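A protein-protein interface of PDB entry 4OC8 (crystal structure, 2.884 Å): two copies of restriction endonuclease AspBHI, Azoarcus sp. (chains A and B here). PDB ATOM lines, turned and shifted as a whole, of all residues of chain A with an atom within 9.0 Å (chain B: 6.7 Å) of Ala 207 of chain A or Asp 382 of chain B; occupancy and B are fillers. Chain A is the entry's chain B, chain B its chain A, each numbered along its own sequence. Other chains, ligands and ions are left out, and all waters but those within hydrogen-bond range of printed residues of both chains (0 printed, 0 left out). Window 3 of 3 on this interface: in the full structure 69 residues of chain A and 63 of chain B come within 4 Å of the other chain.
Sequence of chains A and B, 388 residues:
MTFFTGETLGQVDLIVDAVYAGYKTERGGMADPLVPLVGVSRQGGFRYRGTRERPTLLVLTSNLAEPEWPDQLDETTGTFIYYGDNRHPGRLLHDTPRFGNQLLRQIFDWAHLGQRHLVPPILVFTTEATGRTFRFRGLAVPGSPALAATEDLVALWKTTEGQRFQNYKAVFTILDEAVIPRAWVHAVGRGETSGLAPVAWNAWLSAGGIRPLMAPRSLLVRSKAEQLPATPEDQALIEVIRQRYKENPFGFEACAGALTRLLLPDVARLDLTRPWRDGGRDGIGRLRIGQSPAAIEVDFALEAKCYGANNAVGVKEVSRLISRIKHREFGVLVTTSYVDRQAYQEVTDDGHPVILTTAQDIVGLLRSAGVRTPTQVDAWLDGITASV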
ATOM      1  N   ARG A 116       0.231  18.566  22.292  1.00  0.00           N
ATOM      2  CA  ARG A 116       1.293  18.353  23.266  1.00  0.00           C
ATOM      3  C   ARG A 116       2.562  19.153  22.975  1.00  0.00           C
ATOM      4  O   ARG A 116       3.470  19.223  23.805  1.00  0.00           O
ATOM      5  CB  ARG A 116       1.583  16.857  23.403  1.00  0.00           C
ATOM      6  CG  ARG A 116       0.362  16.069  23.866  1.00  0.00           C
ATOM      7  CD  ARG A 116       0.661  14.598  24.081  1.00  0.00           C
ATOM      8  NE  ARG A 116       1.073  13.955  22.840  1.00  0.00           N
ATOM      9  CZ  ARG A 116       0.228  13.457  21.943  1.00  0.00           C
ATOM     10  NH1 ARG A 116      -1.078  13.527  22.153  1.00  0.00           N
ATOM     11  NH2 ARG A 116       0.690  12.892  20.837  1.00  0.00           N
ATOM     12  N   VAL A 199      14.547  10.829  24.832  1.00  0.00           N
ATOM     13  CA  VAL A 199      13.754   9.934  24.002  1.00  0.00           C
ATOM     14  C   VAL A 199      12.325   9.767  24.505  1.00  0.00           C
ATOM     15  O   VAL A 199      11.378   9.788  23.717  1.00  0.00           O
ATOM     16  CB  VAL A 199      14.414   8.558  23.889  1.00  0.00           C
ATOM     17  CG1 VAL A 199      13.642   7.683  22.919  1.00  0.00           C
ATOM     18  CG2 VAL A 199      15.854   8.718  23.443  1.00  0.00           C
ATOM     19  N   ALA A 200      12.174   9.607  25.815  1.00  0.00           N
ATOM     20  CA  ALA A 200      10.859   9.415  26.413  1.00  0.00           C
ATOM     21  C   ALA A 200       9.975  10.636  26.181  1.00  0.00           C
ATOM     22  O   ALA A 200       8.757  10.517  25.991  1.00  0.00           O
ATOM     23  CB  ALA A 200      10.992   9.126  27.893  1.00  0.00           C
ATOM     24  N   TRP A 201      10.597  11.811  26.179  1.00  0.00           N
ATOM     25  CA  TRP A 201       9.865  13.041  25.916  1.00  0.00           C
ATOM     26  C   TRP A 201       9.337  13.096  24.487  1.00  0.00           C
ATOM     27  O   TRP A 201       8.159  13.356  24.284  1.00  0.00           O
ATOM     28  CB  TRP A 201      10.704  14.279  26.212  1.00  0.00           C
ATOM     29  CG  TRP A 201       9.933  15.531  25.975  1.00  0.00           C
ATOM     30  CD1 TRP A 201       9.966  16.316  24.863  1.00  0.00           C
ATOM     31  CD2 TRP A 201       8.982  16.130  26.862  1.00  0.00           C
ATOM     32  NE1 TRP A 201       9.106  17.379  25.005  1.00  0.00           N
ATOM     33  CE2 TRP A 201       8.490  17.286  26.226  1.00  0.00           C
ATOM     34  CE3 TRP A 201       8.502  15.804  28.134  1.00  0.00           C
ATOM     35  CZ2 TRP A 201       7.544  18.117  26.819  1.00  0.00           C
ATOM     36  CZ3 TRP A 201       7.561  16.631  28.721  1.00  0.00           C
ATOM     37  CH2 TRP A 201       7.094  17.773  28.064  1.00  0.00           C
ATOM     38  N   ASN A 202      10.206  12.859  23.505  1.00  0.00           N
ATOM     39  CA  ASN A 202       9.775  12.793  22.107  1.00  0.00           C
ATOM     40  C   ASN A 202       8.676  11.755  21.929  1.00  0.00           C
ATOM     41  O   ASN A 202       7.692  11.991  21.231  1.00  0.00           O
ATOM     42  CB  ASN A 202      10.945  12.465  21.173  1.00  0.00           C
ATOM     43  CG  ASN A 202      11.864  13.646  20.943  1.00  0.00           C
ATOM     44  OD1 ASN A 202      11.454  14.801  21.056  1.00  0.00           O
ATOM     45  ND2 ASN A 202      13.119  13.362  20.612  1.00  0.00           N
ATOM     46  N   ALA A 203       8.857  10.605  22.569  1.00  0.00           N
ATOM     47  CA  ALA A 203       7.873   9.533  22.532  1.00  0.00           C
ATOM     48  C   ALA A 203       6.505  10.028  23.018  1.00  0.00           C
ATOM     49  O   ALA A 203       5.470   9.784  22.372  1.00  0.00           O
ATOM     50  CB  ALA A 203       8.355   8.359  23.366  1.00  0.00           C
ATOM     51  N   TRP A 204       6.501  10.739  24.142  1.00  0.00           N
ATOM     52  CA  TRP A 204       5.257  11.311  24.645  1.00  0.00           C
ATOM     53  C   TRP A 204       4.676  12.372  23.698  1.00  0.00           C
ATOM     54  O   TRP A 204       3.460  12.460  23.531  1.00  0.00           O
ATOM     55  CB  TRP A 204       5.434  11.883  26.055  1.00  0.00           C
ATOM     56  CG  TRP A 204       4.192  12.543  26.552  1.00  0.00           C
ATOM     57  CD1 TRP A 204       3.092  11.930  27.079  1.00  0.00           C
ATOM     58  CD2 TRP A 204       3.907  13.944  26.548  1.00  0.00           C
ATOM     59  NE1 TRP A 204       2.143  12.865  27.409  1.00  0.00           N
ATOM     60  CE2 TRP A 204       2.619  14.112  27.090  1.00  0.00           C
ATOM     61  CE3 TRP A 204       4.617  15.077  26.140  1.00  0.00           C
ATOM     62  CZ2 TRP A 204       2.026  15.362  27.236  1.00  0.00           C
ATOM     63  CZ3 TRP A 204       4.027  16.318  26.282  1.00  0.00           C
ATOM     64  CH2 TRP A 204       2.745  16.452  26.825  1.00  0.00           C
ATOM     65  N   LEU A 205       5.545  13.169  23.082  1.00  0.00           N
ATOM     66  CA  LEU A 205       5.118  14.207  22.145  1.00  0.00           C
ATOM     67  C   LEU A 205       4.404  13.618  20.938  1.00  0.00           C
ATOM     68  O   LEU A 205       3.350  14.109  20.521  1.00  0.00           O
ATOM     69  CB  LEU A 205       6.315  15.027  21.662  1.00  0.00           C
ATOM     70  CG  LEU A 205       6.762  16.190  22.540  1.00  0.00           C
ATOM     71  CD1 LEU A 205       7.932  16.915  21.902  1.00  0.00           C
ATOM     72  CD2 LEU A 205       5.604  17.138  22.761  1.00  0.00           C
ATOM     73  N   SER A 206       4.990  12.563  20.380  1.00  0.00           N
ATOM     74  CA  SER A 206       4.448  11.929  19.191  1.00  0.00           C
ATOM     75  C   SER A 206       3.224  11.077  19.497  1.00  0.00           C
ATOM     76  O   SER A 206       2.130  11.364  19.013  1.00  0.00           O
ATOM     77  CB  SER A 206       5.514  11.083  18.494  1.00  0.00           C
ATOM     78  OG  SER A 206       6.110  10.167  19.393  1.00  0.00           O
ATOM     79  N   ALA A 207       3.405  10.039  20.308  1.00  0.00           N
ATOM     80  CA  ALA A 207       2.361   9.028  20.462  1.00  0.00           C
ATOM     81  C   ALA A 207       1.443   9.262  21.661  1.00  0.00           C
ATOM     82  O   ALA A 207       0.360   8.683  21.741  1.00  0.00           O
ATOM     83  CB  ALA A 207       2.978   7.632  20.520  1.00  0.00           C
ATOM     84  N   GLY A 208       1.875  10.112  22.589  1.00  0.00           N
ATOM     85  CA  GLY A 208       1.112  10.364  23.798  1.00  0.00           C
ATOM     86  C   GLY A 208       1.371   9.309  24.860  1.00  0.00           C
ATOM     87  O   GLY A 208       0.738   9.301  25.922  1.00  0.00           O
ATOM     88  N   GLY A 209       2.310   8.414  24.574  1.00  0.00           N
ATOM     89  CA  GLY A 209       2.638   7.338  25.489  1.00  0.00           C
ATOM     90  C   GLY A 209       3.526   7.793  26.629  1.00  0.00           C
ATOM     91  O   GLY A 209       4.375   8.669  26.459  1.00  0.00           O
ATOM     92  N   ILE A 210       3.333   7.191  27.798  1.00  0.00           N
ATOM     93  CA  ILE A 210       4.115   7.548  28.972  1.00  0.00           C
ATOM     94  C   ILE A 210       4.971   6.378  29.431  1.00  0.00           C
ATOM     95  O   ILE A 210       4.455   5.301  29.723  1.00  0.00           O
ATOM     96  CB  ILE A 210       3.212   7.993  30.128  1.00  0.00           C
ATOM     97  CG1 ILE A 210       2.421   9.239  29.733  1.00  0.00           C
ATOM     98  CG2 ILE A 210       4.037   8.264  31.373  1.00  0.00           C
ATOM     99  CD1 ILE A 210       1.459   9.702  30.793  1.00  0.00           C
ATOM    100  N   ARG A 211       6.281   6.600  29.486  1.00  0.00           N
ATOM    101  CA  ARG A 211       7.229   5.590  29.945  1.00  0.00           C
ATOM    102  C   ARG A 211       7.760   6.001  31.318  1.00  0.00           C
ATOM    103  O   ARG A 211       8.793   6.659  31.419  1.00  0.00           O
ATOM    104  CB  ARG A 211       8.382   5.441  28.941  1.00  0.00           C
ATOM    105  CG  ARG A 211       9.354   4.300  29.243  1.00  0.00           C
ATOM    106  CD  ARG A 211      10.580   4.319  28.324  1.00  0.00           C
ATOM    107  NE  ARG A 211      10.254   3.995  26.934  1.00  0.00           N
ATOM    108  CZ  ARG A 211      10.487   4.800  25.898  1.00  0.00           C
ATOM    109  NH1 ARG A 211      11.055   5.985  26.085  1.00  0.00           N
ATOM    110  NH2 ARG A 211      10.157   4.421  24.669  1.00  0.00           N
ATOM    111  N   ARG B 244      -3.825  -5.203  15.359  1.00  0.00           N
ATOM    112  CA  ARG B 244      -2.519  -4.630  15.675  1.00  0.00           C
ATOM    113  C   ARG B 244      -1.449  -5.691  15.952  1.00  0.00           C
ATOM    114  O   ARG B 244      -0.271  -5.486  15.648  1.00  0.00           O
ATOM    115  CB  ARG B 244      -2.629  -3.665  16.861  1.00  0.00           C
ATOM    116  CG  ARG B 244      -1.304  -3.070  17.324  1.00  0.00           C
ATOM    117  CD  ARG B 244      -0.655  -2.245  16.233  1.00  0.00           C
ATOM    118  NE  ARG B 244      -1.400  -1.021  15.965  1.00  0.00           N
ATOM    119  CZ  ARG B 244      -0.945   0.198  16.228  1.00  0.00           C
ATOM    120  NH1 ARG B 244       0.265   0.357  16.756  1.00  0.00           N
ATOM    121  NH2 ARG B 244      -1.696   1.260  15.955  1.00  0.00           N
ATOM    122  N   TYR B 245      -1.853  -6.825  16.514  1.00  0.00           N
ATOM    123  CA  TYR B 245      -0.873  -7.816  16.955  1.00  0.00           C
ATOM    124  C   TYR B 245      -0.857  -9.125  16.155  1.00  0.00           C
ATOM    125  O   TYR B 245      -0.292 -10.128  16.604  1.00  0.00           O
ATOM    126  CB  TYR B 245      -1.030  -8.087  18.455  1.00  0.00           C
ATOM    127  CG  TYR B 245      -0.714  -6.873  19.292  1.00  0.00           C
ATOM    128  CD1 TYR B 245       0.603  -6.523  19.571  1.00  0.00           C
ATOM    129  CD2 TYR B 245      -1.728  -6.061  19.787  1.00  0.00           C
ATOM    130  CE1 TYR B 245       0.898  -5.403  20.326  1.00  0.00           C
ATOM    131  CE2 TYR B 245      -1.441  -4.939  20.546  1.00  0.00           C
ATOM    132  CZ  TYR B 245      -0.127  -4.616  20.812  1.00  0.00           C
ATOM    133  OH  TYR B 245       0.165  -3.500  21.563  1.00  0.00           O
ATOM    134  N   THR B 375      -9.588   5.329  15.806  1.00  0.00           N
ATOM    135  CA  THR B 375      -8.406   6.174  15.672  1.00  0.00           C
ATOM    136  C   THR B 375      -7.734   6.332  17.030  1.00  0.00           C
ATOM    137  O   THR B 375      -6.504   6.247  17.149  1.00  0.00           O
ATOM    138  CB  THR B 375      -8.754   7.569  15.130  1.00  0.00           C
ATOM    139  OG1 THR B 375      -9.795   7.461  14.150  1.00  0.00           O
ATOM    140  CG2 THR B 375      -7.521   8.218  14.507  1.00  0.00           C
ATOM    141  N   VAL B 377      -8.001   4.259  19.559  1.00  0.00           N
ATOM    142  CA  VAL B 377      -7.409   2.960  19.869  1.00  0.00           C
ATOM    143  C   VAL B 377      -6.036   2.853  19.214  1.00  0.00           C
ATOM    144  O   VAL B 377      -5.076   2.392  19.834  1.00  0.00           O
ATOM    145  CB  VAL B 377      -8.286   1.789  19.374  1.00  0.00           C
ATOM    146  CG1 VAL B 377      -7.591   0.463  19.625  1.00  0.00           C
ATOM    147  CG2 VAL B 377      -9.640   1.805  20.049  1.00  0.00           C
ATOM    148  N   ASP B 378      -5.953   3.293  17.960  1.00  0.00           N
ATOM    149  CA  ASP B 378      -4.690   3.266  17.224  1.00  0.00           C
ATOM    150  C   ASP B 378      -3.614   4.104  17.905  1.00  0.00           C
ATOM    151  O   ASP B 378      -2.485   3.638  18.103  1.00  0.00           O
ATOM    152  CB  ASP B 378      -4.892   3.725  15.778  1.00  0.00           C
ATOM    153  CG  ASP B 378      -5.323   2.593  14.865  1.00  0.00           C
ATOM    154  OD1 ASP B 378      -4.859   1.452  15.080  1.00  0.00           O
ATOM    155  OD2 ASP B 378      -6.122   2.842  13.934  1.00  0.00           O
ATOM    156  N   ALA B 379      -3.968   5.334  18.268  1.00  0.00           N
ATOM    157  CA  ALA B 379      -3.040   6.221  18.967  1.00  0.00           C
ATOM    158  C   ALA B 379      -2.599   5.619  20.300  1.00  0.00           C
ATOM    159  O   ALA B 379      -1.424   5.698  20.674  1.00  0.00           O
ATOM    160  CB  ALA B 379      -3.677   7.571  19.186  1.00  0.00           C
ATOM    161  N   TRP B 380      -3.554   5.016  21.006  1.00  0.00           N
ATOM    162  CA  TRP B 380      -3.299   4.367  22.282  1.00  0.00           C
ATOM    163  C   TRP B 380      -2.271   3.247  22.138  1.00  0.00           C
ATOM    164  O   TRP B 380      -1.305   3.168  22.911  1.00  0.00           O
ATOM    165  CB  TRP B 380      -4.606   3.817  22.855  1.00  0.00           C
ATOM    166  CG  TRP B 380      -4.447   3.096  24.159  1.00  0.00           C
ATOM    167  CD1 TRP B 380      -4.112   3.643  25.360  1.00  0.00           C
ATOM    168  CD2 TRP B 380      -4.631   1.696  24.394  1.00  0.00           C
ATOM    169  NE1 TRP B 380      -4.064   2.672  26.326  1.00  0.00           N
ATOM    170  CE2 TRP B 380      -4.381   1.464  25.758  1.00  0.00           C
ATOM    171  CE3 TRP B 380      -4.981   0.610  23.583  1.00  0.00           C
ATOM    172  CZ2 TRP B 380      -4.470   0.200  26.334  1.00  0.00           C
ATOM    173  CZ3 TRP B 380      -5.068  -0.647  24.154  1.00  0.00           C
ATOM    174  CH2 TRP B 380      -4.816  -0.841  25.516  1.00  0.00           C
ATOM    175  N   LEU B 381      -2.484   2.390  21.141  1.00  0.00           N
ATOM    176  CA  LEU B 381      -1.569   1.290  20.852  1.00  0.00           C
ATOM    177  C   LEU B 381      -0.185   1.797  20.444  1.00  0.00           C
ATOM    178  O   LEU B 381       0.839   1.218  20.829  1.00  0.00           O
ATOM    179  CB  LEU B 381      -2.154   0.386  19.768  1.00  0.00           C
ATOM    180  CG  LEU B 381      -3.353  -0.449  20.212  1.00  0.00           C
ATOM    181  CD1 LEU B 381      -4.011  -1.136  19.032  1.00  0.00           C
ATOM    182  CD2 LEU B 381      -2.931  -1.472  21.252  1.00  0.00           C
ATOM    183  N   ASP B 382      -0.158   2.876  19.666  1.00  0.00           N
ATOM    184  CA  ASP B 382       1.100   3.521  19.311  1.00  0.00           C
ATOM    185  C   ASP B 382       1.834   3.917  20.587  1.00  0.00           C
ATOM    186  O   ASP B 382       3.046   3.701  20.721  1.00  0.00           O
ATOM    187  CB  ASP B 382       0.854   4.750  18.431  1.00  0.00           C
ATOM    188  CG  ASP B 382       0.417   4.383  17.019  1.00  0.00           C
ATOM    189  OD1 ASP B 382       0.865   3.333  16.506  1.00  0.00           O
ATOM    190  OD2 ASP B 382      -0.371   5.150  16.424  1.00  0.00           O
ATOM    191  N   GLY B 383       1.076   4.476  21.527  1.00  0.00           N
ATOM    192  CA  GLY B 383       1.596   4.838  22.832  1.00  0.00           C
ATOM    193  C   GLY B 383       2.192   3.659  23.576  1.00  0.00           C
ATOM    194  O   GLY B 383       3.306   3.746  24.096  1.00  0.00           O
ATOM    195  N   ILE B 384       1.456   2.552  23.626  1.00  0.00           N
ATOM    196  CA  ILE B 384       1.947   1.356  24.309  1.00  0.00           C
ATOM    197  C   ILE B 384       3.248   0.857  23.697  1.00  0.00           C
ATOM    198  O   ILE B 384       4.236   0.675  24.404  1.00  0.00           O
ATOM    199  CB  ILE B 384       0.935   0.205  24.260  1.00  0.00           C
ATOM    200  CG1 ILE B 384      -0.427   0.664  24.766  1.00  0.00           C
ATOM    201  CG2 ILE B 384       1.438  -0.985  25.072  1.00  0.00           C
ATOM    202  CD1 ILE B 384      -1.484  -0.404  24.651  1.00  0.00           C
ATOM    203  N   THR B 385       3.240   0.636  22.385  1.00  0.00           N
ATOM    204  CA  THR B 385       4.413   0.093  21.699  1.00  0.00           C
ATOM    205  C   THR B 385       5.623   1.010  21.836  1.00  0.00           C
ATOM    206  O   THR B 385       6.750   0.541  21.997  1.00  0.00           O
ATOM    207  CB  THR B 385       4.138  -0.181  20.206  1.00  0.00           C
ATOM    208  OG1 THR B 385       3.788   1.043  19.550  1.00  0.00           O
ATOM    209  CG2 THR B 385       2.999  -1.186  20.044  1.00  0.00           C
ATOM    210  N   ALA B 386       5.382   2.317  21.793  1.00  0.00           N
ATOM    211  CA  ALA B 386       6.464   3.290  21.918  1.00  0.00           C
ATOM    212  C   ALA B 386       6.988   3.418  23.348  1.00  0.00           C
ATOM    213  O   ALA B 386       8.151   3.765  23.557  1.00  0.00           O
ATOM    214  CB  ALA B 386       6.025   4.650  21.390  1.00  0.00           C
ATOM    215  N   SER B 387       6.134   3.137  24.328  1.00  0.00           N
ATOM    216  CA  SER B 387       6.503   3.320  25.731  1.00  0.00           C
ATOM    217  C   SER B 387       7.027   2.045  26.387  1.00  0.00           C
ATOM    218  O   SER B 387       7.287   2.024  27.591  1.00  0.00           O
ATOM    219  CB  SER B 387       5.328   3.879  26.536  1.00  0.00           C
ATOM    220  OG  SER B 387       4.254   2.958  26.569  1.00  0.00           O
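Among the printed residues, merely in contact across the chains: Arg 211 of chain A with Ser 387 of chain B (3.5 Å), Ile 210 of chain A with Ser 387 of chain B (3.6 Å), Ala 207 of chain A with Ala 379 of chain B (3.6 Å), Gly 209 of chain A with Gly 383 of chain B (3.8 Å), Ala 207 of chain A with Gly 383 of chain B (3.8 Å) and Ala 207 of chain A with Asp 382 of chain B (3.9 Å).
No position is printed for both chains.
Of the 7 pairs that touch across the chains among the printed residues, none has its exchanged pair printed and touching as well.
The backbone carbonyl oxygen (O) of Ala 386 of chain B sits close to the guanidinium group (NH2) of Arg 211 of chain A (2.4 Å).
Asp 382 of chain B touches one residue of chain A.
Printed residues of chain A within 4 Å of Gly 383 of chain B: Ala 207 and Gly 209.
Of the printed residues of chain A, Ser 387 of chain B touches Ile 210 (3.6 Å) and Arg 211 (3.5 Å).
Printed residues of chain B within 4 Å of Ile 210 of chain A: Ser 387 (3.6 Å).
Printed residues of chain B within 4 Å of Arg 211 of chain A: Ala 386 and Ser 387.
Of the printed residues of chain A, Ala 386 of chain B touches Arg 211.
Leu 205 of chain A touches none of the printed residues of chain B.
Val 377 of chain B touches none of the printed residues of chain A.
The nearest residue of chain B that does not touch Ala 207 of chain A is Ala 386 of chain B (4.4 Å).
The nearest residue of chain A that does not touch Asp 382 of chain B is Gly 209 of chain A (6.0 Å).
The side-chain hydroxyl of Thr 385 of chain B lies within hydrogen-bond range of the backbone carbonyl oxygen of Asp 382 of chain B.
The side-chain carboxylate (OD1) of Asp 382 of chain B is in salt-bridge range of the guanidinium group (NH1) of Arg 244 of chain B (3.0 Å).
OG of Ser 387 of chain B sits at hydrogen-bond distance from O of Gly 383 of chain B (2.8 Å).
O of Ile 384 of chain B sits at hydrogen-bond distance from OG of Ser 387 of chain B, at 3.1 Å.
Of the 14 printed residues of chain A, 4 touch a printed residue of chain B.
Hydrophobic or aromatic side chains of chain A within 4 Å of the printed part of chain B: Ala 207.
Among the printed residues, 7 pairs touch across the chains.
Among the printed residues, no Asp or Glu carboxylate lies within 4 Å of a Lys or Arg side-chain nitrogen of the other chain.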
